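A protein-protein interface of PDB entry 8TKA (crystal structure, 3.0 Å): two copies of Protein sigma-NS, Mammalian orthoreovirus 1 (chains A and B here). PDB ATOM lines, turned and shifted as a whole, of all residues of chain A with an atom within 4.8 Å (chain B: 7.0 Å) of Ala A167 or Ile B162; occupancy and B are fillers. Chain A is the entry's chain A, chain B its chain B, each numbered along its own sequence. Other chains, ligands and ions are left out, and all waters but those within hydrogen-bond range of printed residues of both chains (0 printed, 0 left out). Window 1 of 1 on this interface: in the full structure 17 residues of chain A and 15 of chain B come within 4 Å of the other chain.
A ring nitrogen (NE2) of His A164 sits at hydrogen-bond distance from the backbone carbonyl oxygen of Gly B148, 3.1 Å away. A ring nitrogen (NE2) of His A164 is in hydrogen-bond range of the backbone carbonyl oxygen of Val B160 (2.8 Å). OD1 of Asp A168 is in salt-bridge range of NH1 of Arg B67 (3.1 Å).
The backbone NH (N) of Val B160 lies within hydrogen-bond range of the backbone carbonyl oxygen (O) of Gly B148 (3.0 Å).
NE2 of His B164 touches CG1 of Ile A162 (3.8 Å). Ala B167 touches Ile A162 (CB to CD1, 3.97 Å). CD1 of Ile B162 touches O of Met A163 (3.9 Å). His A164 touches Arg B67. CG1 of Ile B162 touches NE2 of His A164 (3.8 Å). Arg B67 touches Ala A167. Ile B162 touches Ala A167. Leu B68 touches Asp A168.
Of chain B, only Arg B67 and Ile B162 come within 4 Å of Ala A167. Printed residues of chain A within 4 Å of Ile B162: Met A163 (3.9 Å), His A164 (3.8 Å) and Ala A167 (3.8 Å). Printed residues of chain A within 4 Å of Leu B68: Asp A168 (3.6 Å). Of the printed residues of chain B, His A164 touches Arg B67, Gly B148, Val B160 and Ile B162. Printed residues of chain B within 4 Å of Met A163: Ile B162. Of the printed residues of chain A, Gly B148 touches His A164 (3.1 Å). Of the printed residues of chain A, Val B160 touches His A164. Leu B149 touches none of the printed residues of chain A.
Of the 18 printed residues of chain B, 7 touch a printed residue of chain A. Hydrophobic or aromatic side chains of chain B that line the printed part of chain A: Leu B68, Ile B162, His B164 and Ala B167. Of the 10 printed residues of chain A, 5 touch a printed residue of chain B. Hydrophobic or aromatic side chains of chain A within 4 Å of the printed part of chain B: Ile A162, His A164 and Ala A167. Among the printed residues, 11 pairs touch across the chains.
Ile A162 touches His B164, and with the chains exchanged His A164 touches Ile B162. Ile A162 touches Ala B167, and with the chains exchanged Ala A167 touches Ile B162. Met A163 touches Ile B162, but with the chains exchanged Ile A162 does not touch Met B163 (4.2 Å). Positions printed for both chains: 60, 162, 163, 164, 165, 166 and 167. Of the 11 pairs that touch across the chains among the printed residues, 4 have their exchanged pair printed and touching as well.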
ATOM      1  N   LEU A  60     -11.737  17.063  -5.759  1.00  0.00           N
ATOM      2  CA  LEU A  60     -10.682  16.062  -5.841  1.00  0.00           C
ATOM      3  C   LEU A  60      -9.290  16.661  -5.542  1.00  0.00           C
ATOM      4  O   LEU A  60      -8.460  16.043  -4.882  1.00  0.00           O
ATOM      5  CB  LEU A  60     -10.738  15.338  -7.196  1.00  0.00           C
ATOM      6  CG  LEU A  60     -11.915  14.393  -7.509  1.00  0.00           C
ATOM      7  CD1 LEU A  60     -11.769  13.812  -8.912  1.00  0.00           C
ATOM      8  CD2 LEU A  60     -12.084  13.279  -6.474  1.00  0.00           C
ATOM      9  N   ILE A 162     -17.615   8.607  -5.095  1.00  0.00           N
ATOM     10  CA  ILE A 162     -17.018   9.804  -5.691  1.00  0.00           C
ATOM     11  C   ILE A 162     -17.994  10.332  -6.734  1.00  0.00           C
ATOM     12  O   ILE A 162     -18.463   9.572  -7.568  1.00  0.00           O
ATOM     13  CB  ILE A 162     -15.679   9.470  -6.396  1.00  0.00           C
ATOM     14  CG1 ILE A 162     -14.723   8.796  -5.400  1.00  0.00           C
ATOM     15  CG2 ILE A 162     -15.042  10.707  -7.034  1.00  0.00           C
ATOM     16  CD1 ILE A 162     -13.370   8.388  -5.947  1.00  0.00           C
ATOM     17  N   MET A 163     -18.259  11.632  -6.710  1.00  0.00           N
ATOM     18  CA  MET A 163     -19.200  12.266  -7.632  1.00  0.00           C
ATOM     19  C   MET A 163     -18.587  12.504  -8.981  1.00  0.00           C
ATOM     20  O   MET A 163     -17.447  12.923  -9.083  1.00  0.00           O
ATOM     21  CB  MET A 163     -19.634  13.634  -7.088  1.00  0.00           C
ATOM     22  CG  MET A 163     -20.378  13.566  -5.747  1.00  0.00           C
ATOM     23  SD  MET A 163     -22.063  12.473  -5.835  1.00  0.00           S
ATOM     24  CE  MET A 163     -23.248  13.551  -7.056  1.00  0.00           C
ATOM     25  N   HIS A 164     -19.368  12.288 -10.027  1.00  0.00           N
ATOM     26  CA  HIS A 164     -18.927  12.496 -11.401  1.00  0.00           C
ATOM     27  C   HIS A 164     -18.667  13.943 -11.766  1.00  0.00           C
ATOM     28  O   HIS A 164     -17.911  14.222 -12.679  1.00  0.00           O
ATOM     29  CB  HIS A 164     -19.938  11.889 -12.382  1.00  0.00           C
ATOM     30  CG  HIS A 164     -19.974  10.392 -12.337  1.00  0.00           C
ATOM     31  ND1 HIS A 164     -20.434   9.691 -11.241  1.00  0.00           N
ATOM     32  CD2 HIS A 164     -19.578   9.462 -13.242  1.00  0.00           C
ATOM     33  CE1 HIS A 164     -20.324   8.398 -11.478  1.00  0.00           C
ATOM     34  NE2 HIS A 164     -19.812   8.230 -12.685  1.00  0.00           N
ATOM     35  N   LEU A 165     -19.281  14.865 -11.055  1.00  0.00           N
ATOM     36  CA  LEU A 165     -19.033  16.290 -11.263  1.00  0.00           C
ATOM     37  C   LEU A 165     -17.637  16.672 -10.777  1.00  0.00           C
ATOM     38  O   LEU A 165     -16.949  17.450 -11.425  1.00  0.00           O
ATOM     39  CB  LEU A 165     -20.113  17.125 -10.554  1.00  0.00           C
ATOM     40  CG  LEU A 165     -20.029  18.633 -10.744  1.00  0.00           C
ATOM     41  CD1 LEU A 165     -20.537  19.043 -12.116  1.00  0.00           C
ATOM     42  CD2 LEU A 165     -20.788  19.333  -9.635  1.00  0.00           C
ATOM     43  N   ALA A 166     -17.217  16.114  -9.643  1.00  0.00           N
ATOM     44  CA  ALA A 166     -15.886  16.358  -9.120  1.00  0.00           C
ATOM     45  C   ALA A 166     -14.820  15.938 -10.114  1.00  0.00           C
ATOM     46  O   ALA A 166     -13.862  16.659 -10.311  1.00  0.00           O
ATOM     47  CB  ALA A 166     -15.695  15.630  -7.809  1.00  0.00           C
ATOM     48  N   ALA A 167     -15.003  14.775 -10.737  1.00  0.00           N
ATOM     49  CA  ALA A 167     -14.149  14.316 -11.812  1.00  0.00           C
ATOM     50  C   ALA A 167     -14.234  15.185 -13.073  1.00  0.00           C
ATOM     51  O   ALA A 167     -13.196  15.451 -13.702  1.00  0.00           O
ATOM     52  CB  ALA A 167     -14.495  12.890 -12.155  1.00  0.00           C
ATOM     53  N   ASP A 168     -15.453  15.598 -13.446  1.00  0.00           N
ATOM     54  CA  ASP A 168     -15.677  16.485 -14.606  1.00  0.00           C
ATOM     55  C   ASP A 168     -14.942  17.827 -14.489  1.00  0.00           C
ATOM     56  O   ASP A 168     -14.377  18.307 -15.473  1.00  0.00           O
ATOM     57  CB  ASP A 168     -17.178  16.747 -14.841  1.00  0.00           C
ATOM     58  CG  ASP A 168     -17.953  15.510 -15.387  1.00  0.00           C
ATOM     59  OD1 ASP A 168     -17.356  14.661 -16.076  1.00  0.00           O
ATOM     60  OD2 ASP A 168     -19.189  15.385 -15.143  1.00  0.00           O
ATOM     61  N   LEU A 169     -14.931  18.398 -13.286  1.00  0.00           N
ATOM     62  CA  LEU A 169     -14.349  19.725 -13.046  1.00  0.00           C
ATOM     63  C   LEU A 169     -12.856  19.755 -12.760  1.00  0.00           C
ATOM     64  O   LEU A 169     -12.277  20.822 -12.712  1.00  0.00           O
ATOM     65  CB  LEU A 169     -15.068  20.422 -11.877  1.00  0.00           C
ATOM     66  CG  LEU A 169     -16.551  20.719 -12.071  1.00  0.00           C
ATOM     67  CD1 LEU A 169     -17.119  21.290 -10.776  1.00  0.00           C
ATOM     68  CD2 LEU A 169     -16.789  21.641 -13.262  1.00  0.00           C
ATOM     69  N   ASP A 170     -12.228  18.605 -12.576  1.00  0.00           N
ATOM     70  CA  ASP A 170     -10.847  18.563 -12.081  1.00  0.00           C
ATOM     71  C   ASP A 170      -9.788  19.033 -13.093  1.00  0.00           C
ATOM     72  O   ASP A 170      -8.670  19.311 -12.720  1.00  0.00           O
ATOM     73  CB  ASP A 170     -10.501  17.168 -11.557  1.00  0.00           C
ATOM     74  CG  ASP A 170      -9.372  17.187 -10.529  1.00  0.00           C
ATOM     75  OD1 ASP A 170      -8.178  17.029 -10.911  1.00  0.00           O
ATOM     76  OD2 ASP A 170      -9.684  17.349  -9.319  1.00  0.00           O
ATOM     77  N   LEU B  60      -8.359   8.257 -14.459  1.00  0.00           N
ATOM     78  CA  LEU B  60      -8.981   9.582 -14.465  1.00  0.00           C
ATOM     79  C   LEU B  60      -8.325  10.541 -15.459  1.00  0.00           C
ATOM     80  O   LEU B  60      -8.991  11.377 -16.031  1.00  0.00           O
ATOM     81  CB  LEU B  60      -9.028  10.181 -13.054  1.00  0.00           C
ATOM     82  CG  LEU B  60     -10.024   9.558 -12.088  1.00  0.00           C
ATOM     83  CD1 LEU B  60      -9.920  10.268 -10.772  1.00  0.00           C
ATOM     84  CD2 LEU B  60     -11.445   9.643 -12.611  1.00  0.00           C
ATOM     85  N   LYS B  64      -9.979  12.191 -18.716  1.00  0.00           N
ATOM     86  CA  LYS B  64     -10.091  13.631 -18.435  1.00  0.00           C
ATOM     87  C   LYS B  64     -10.805  14.495 -19.486  1.00  0.00           C
ATOM     88  O   LYS B  64     -11.792  15.167 -19.161  1.00  0.00           O
ATOM     89  CB  LYS B  64      -8.696  14.188 -18.144  1.00  0.00           C
ATOM     90  CG  LYS B  64      -8.633  15.657 -17.732  1.00  0.00           C
ATOM     91  CD  LYS B  64      -7.211  16.084 -17.378  1.00  0.00           C
ATOM     92  CE  LYS B  64      -6.251  16.063 -18.586  1.00  0.00           C
ATOM     93  NZ  LYS B  64      -6.530  17.077 -19.645  1.00  0.00           N
ATOM     94  N   ARG B  67     -14.544  12.939 -20.949  1.00  0.00           N
ATOM     95  CA  ARG B  67     -15.728  12.968 -20.066  1.00  0.00           C
ATOM     96  C   ARG B  67     -16.536  14.257 -20.185  1.00  0.00           C
ATOM     97  O   ARG B  67     -17.686  14.296 -19.782  1.00  0.00           O
ATOM     98  CB  ARG B  67     -15.344  12.721 -18.604  1.00  0.00           C
ATOM     99  CG  ARG B  67     -14.383  13.730 -18.009  1.00  0.00           C
ATOM    100  CD  ARG B  67     -14.263  13.578 -16.516  1.00  0.00           C
ATOM    101  NE  ARG B  67     -14.101  12.184 -16.118  1.00  0.00           N
ATOM    102  CZ  ARG B  67     -15.028  11.420 -15.539  1.00  0.00           C
ATOM    103  NH1 ARG B  67     -16.247  11.857 -15.242  1.00  0.00           N
ATOM    104  NH2 ARG B  67     -14.718  10.180 -15.235  1.00  0.00           N
ATOM    105  N   LEU B  68     -15.900  15.309 -20.699  1.00  0.00           N
ATOM    106  CA  LEU B  68     -16.553  16.569 -21.012  1.00  0.00           C
ATOM    107  C   LEU B  68     -16.975  16.690 -22.471  1.00  0.00           C
ATOM    108  O   LEU B  68     -17.370  17.762 -22.901  1.00  0.00           O
ATOM    109  CB  LEU B  68     -15.655  17.750 -20.609  1.00  0.00           C
ATOM    110  CG  LEU B  68     -15.828  18.205 -19.162  1.00  0.00           C
ATOM    111  CD1 LEU B  68     -14.852  19.337 -18.891  1.00  0.00           C
ATOM    112  CD2 LEU B  68     -17.263  18.661 -18.878  1.00  0.00           C
ATOM    113  N   TYR B 115     -18.522  -6.457 -13.728  1.00  0.00           N
ATOM    114  CA  TYR B 115     -18.107  -5.086 -13.456  1.00  0.00           C
ATOM    115  C   TYR B 115     -19.196  -4.111 -13.849  1.00  0.00           C
ATOM    116  O   TYR B 115     -19.576  -3.277 -13.040  1.00  0.00           O
ATOM    117  CB  TYR B 115     -16.782  -4.749 -14.175  1.00  0.00           C
ATOM    118  CG  TYR B 115     -16.161  -3.439 -13.727  1.00  0.00           C
ATOM    119  CD1 TYR B 115     -15.817  -3.254 -12.416  1.00  0.00           C
ATOM    120  CD2 TYR B 115     -15.951  -2.383 -14.609  1.00  0.00           C
ATOM    121  CE1 TYR B 115     -15.276  -2.071 -11.968  1.00  0.00           C
ATOM    122  CE2 TYR B 115     -15.412  -1.190 -14.172  1.00  0.00           C
ATOM    123  CZ  TYR B 115     -15.081  -1.047 -12.839  1.00  0.00           C
ATOM    124  OH  TYR B 115     -14.548   0.104 -12.324  1.00  0.00           O
ATOM    125  N   GLY B 145     -14.290   2.635 -17.425  1.00  0.00           N
ATOM    126  CA  GLY B 145     -15.180   2.185 -16.366  1.00  0.00           C
ATOM    127  C   GLY B 145     -14.696   2.466 -14.970  1.00  0.00           C
ATOM    128  O   GLY B 145     -15.498   2.761 -14.099  1.00  0.00           O
ATOM    129  N   MET B 146     -13.391   2.370 -14.753  1.00  0.00           N
ATOM    130  CA  MET B 146     -12.800   2.747 -13.474  1.00  0.00           C
ATOM    131  C   MET B 146     -12.900   4.228 -13.267  1.00  0.00           C
ATOM    132  O   MET B 146     -13.030   4.675 -12.132  1.00  0.00           O
ATOM    133  CB  MET B 146     -11.350   2.301 -13.383  1.00  0.00           C
ATOM    134  CG  MET B 146     -11.236   0.788 -13.235  1.00  0.00           C
ATOM    135  SD  MET B 146      -9.387   0.374 -12.758  1.00  0.00           S
ATOM    136  CE  MET B 146      -8.605   0.626 -14.545  1.00  0.00           C
ATOM    137  N   ALA B 147     -12.853   4.990 -14.367  1.00  0.00           N
ATOM    138  CA  ALA B 147     -13.059   6.440 -14.355  1.00  0.00           C
ATOM    139  C   ALA B 147     -14.513   6.874 -14.251  1.00  0.00           C
ATOM    140  O   ALA B 147     -14.780   8.050 -14.151  1.00  0.00           O
ATOM    141  CB  ALA B 147     -12.437   7.062 -15.580  1.00  0.00           C
ATOM    142  N   GLY B 148     -15.449   5.937 -14.273  1.00  0.00           N
ATOM    143  CA  GLY B 148     -16.851   6.220 -14.081  1.00  0.00           C
ATOM    144  C   GLY B 148     -17.688   6.326 -15.341  1.00  0.00           C
ATOM    145  O   GLY B 148     -18.810   6.793 -15.278  1.00  0.00           O
ATOM    146  N   LEU B 149     -17.170   5.866 -16.472  1.00  0.00           N
ATOM    147  CA  LEU B 149     -17.903   5.912 -17.718  1.00  0.00           C
ATOM    148  C   LEU B 149     -17.908   4.553 -18.389  1.00  0.00           C
ATOM    149  O   LEU B 149     -16.858   4.004 -18.709  1.00  0.00           O
ATOM    150  CB  LEU B 149     -17.271   6.912 -18.659  1.00  0.00           C
ATOM    151  CG  LEU B 149     -17.287   8.356 -18.155  1.00  0.00           C
ATOM    152  CD1 LEU B 149     -16.169   9.147 -18.817  1.00  0.00           C
ATOM    153  CD2 LEU B 149     -18.624   9.024 -18.397  1.00  0.00           C
ATOM    154  N   VAL B 160     -21.081   5.158 -14.265  1.00  0.00           N
ATOM    155  CA  VAL B 160     -20.830   3.971 -13.440  1.00  0.00           C
ATOM    156  C   VAL B 160     -19.965   4.470 -12.302  1.00  0.00           C
ATOM    157  O   VAL B 160     -19.359   5.512 -12.450  1.00  0.00           O
ATOM    158  CB  VAL B 160     -20.139   2.904 -14.313  1.00  0.00           C
ATOM    159  CG1 VAL B 160     -19.373   1.842 -13.521  1.00  0.00           C
ATOM    160  CG2 VAL B 160     -21.184   2.230 -15.182  1.00  0.00           C
ATOM    161  N   PRO B 161     -19.942   3.780 -11.152  1.00  0.00           N
ATOM    162  CA  PRO B 161     -19.146   4.281 -10.018  1.00  0.00           C
ATOM    163  C   PRO B 161     -17.658   4.466 -10.275  1.00  0.00           C
ATOM    164  O   PRO B 161     -17.021   3.594 -10.850  1.00  0.00           O
ATOM    165  CB  PRO B 161     -19.343   3.212  -8.953  1.00  0.00           C
ATOM    166  CG  PRO B 161     -20.704   2.728  -9.209  1.00  0.00           C
ATOM    167  CD  PRO B 161     -20.905   2.765 -10.703  1.00  0.00           C
ATOM    168  N   ILE B 162     -17.124   5.593  -9.821  1.00  0.00           N
ATOM    169  CA  ILE B 162     -15.723   5.942 -10.013  1.00  0.00           C
ATOM    170  C   ILE B 162     -14.896   5.248  -8.950  1.00  0.00           C
ATOM    171  O   ILE B 162     -15.209   5.338  -7.770  1.00  0.00           O
ATOM    172  CB  ILE B 162     -15.504   7.467  -9.886  1.00  0.00           C
ATOM    173  CG1 ILE B 162     -16.429   8.217 -10.860  1.00  0.00           C
ATOM    174  CG2 ILE B 162     -14.041   7.814 -10.152  1.00  0.00           C
ATOM    175  CD1 ILE B 162     -16.236   9.717 -10.992  1.00  0.00           C
ATOM    176  N   MET B 163     -13.810   4.603  -9.363  1.00  0.00           N
ATOM    177  CA  MET B 163     -13.004   3.784  -8.448  1.00  0.00           C
ATOM    178  C   MET B 163     -12.076   4.626  -7.634  1.00  0.00           C
ATOM    179  O   MET B 163     -11.399   5.489  -8.175  1.00  0.00           O
ATOM    180  CB  MET B 163     -12.165   2.772  -9.198  1.00  0.00           C
ATOM    181  CG  MET B 163     -13.026   1.801  -9.994  1.00  0.00           C
ATOM    182  SD  MET B 163     -13.624   0.247  -8.967  1.00  0.00           S
ATOM    183  CE  MET B 163     -15.531   0.723  -8.801  1.00  0.00           C
ATOM    184  N   HIS B 164     -12.027   4.375  -6.327  1.00  0.00           N
ATOM    185  CA  HIS B 164     -11.230   5.187  -5.426  1.00  0.00           C
ATOM    186  C   HIS B 164      -9.771   5.116  -5.735  1.00  0.00           C
ATOM    187  O   HIS B 164      -9.079   6.098  -5.622  1.00  0.00           O
ATOM    188  CB  HIS B 164     -11.468   4.791  -3.981  1.00  0.00           C
ATOM    189  CG  HIS B 164     -12.767   5.293  -3.438  1.00  0.00           C
ATOM    190  ND1 HIS B 164     -13.971   4.703  -3.743  1.00  0.00           N
ATOM    191  CD2 HIS B 164     -13.054   6.337  -2.625  1.00  0.00           C
ATOM    192  CE1 HIS B 164     -14.946   5.353  -3.135  1.00  0.00           C
ATOM    193  NE2 HIS B 164     -14.417   6.349  -2.449  1.00  0.00           N
ATOM    194  N   LEU B 165      -9.307   3.954  -6.155  1.00  0.00           N
ATOM    195  CA  LEU B 165      -7.924   3.790  -6.565  1.00  0.00           C
ATOM    196  C   LEU B 165      -7.508   4.751  -7.710  1.00  0.00           C
ATOM    197  O   LEU B 165      -6.372   5.226  -7.755  1.00  0.00           O
ATOM    198  CB  LEU B 165      -7.690   2.338  -6.968  1.00  0.00           C
ATOM    199  CG  LEU B 165      -6.233   1.923  -7.130  1.00  0.00           C
ATOM    200  CD1 LEU B 165      -5.549   1.678  -5.777  1.00  0.00           C
ATOM    201  CD2 LEU B 165      -6.199   0.700  -8.024  1.00  0.00           C
ATOM    202  N   ALA B 166      -8.421   5.046  -8.625  1.00  0.00           N
ATOM    203  CA  ALA B 166      -8.126   5.968  -9.713  1.00  0.00           C
ATOM    204  C   ALA B 166      -7.866   7.370  -9.212  1.00  0.00           C
ATOM    205  O   ALA B 166      -6.987   8.035  -9.730  1.00  0.00           O
ATOM    206  CB  ALA B 166      -9.247   5.979 -10.718  1.00  0.00           C
ATOM    207  N   ALA B 167      -8.628   7.801  -8.212  1.00  0.00           N
ATOM    208  CA  ALA B 167      -8.417   9.101  -7.551  1.00  0.00           C
ATOM    209  C   ALA B 167      -7.164   9.124  -6.692  1.00  0.00           C
ATOM    210  O   ALA B 167      -6.453  10.141  -6.660  1.00  0.00           O
ATOM    211  CB  ALA B 167      -9.634   9.486  -6.706  1.00  0.00           C
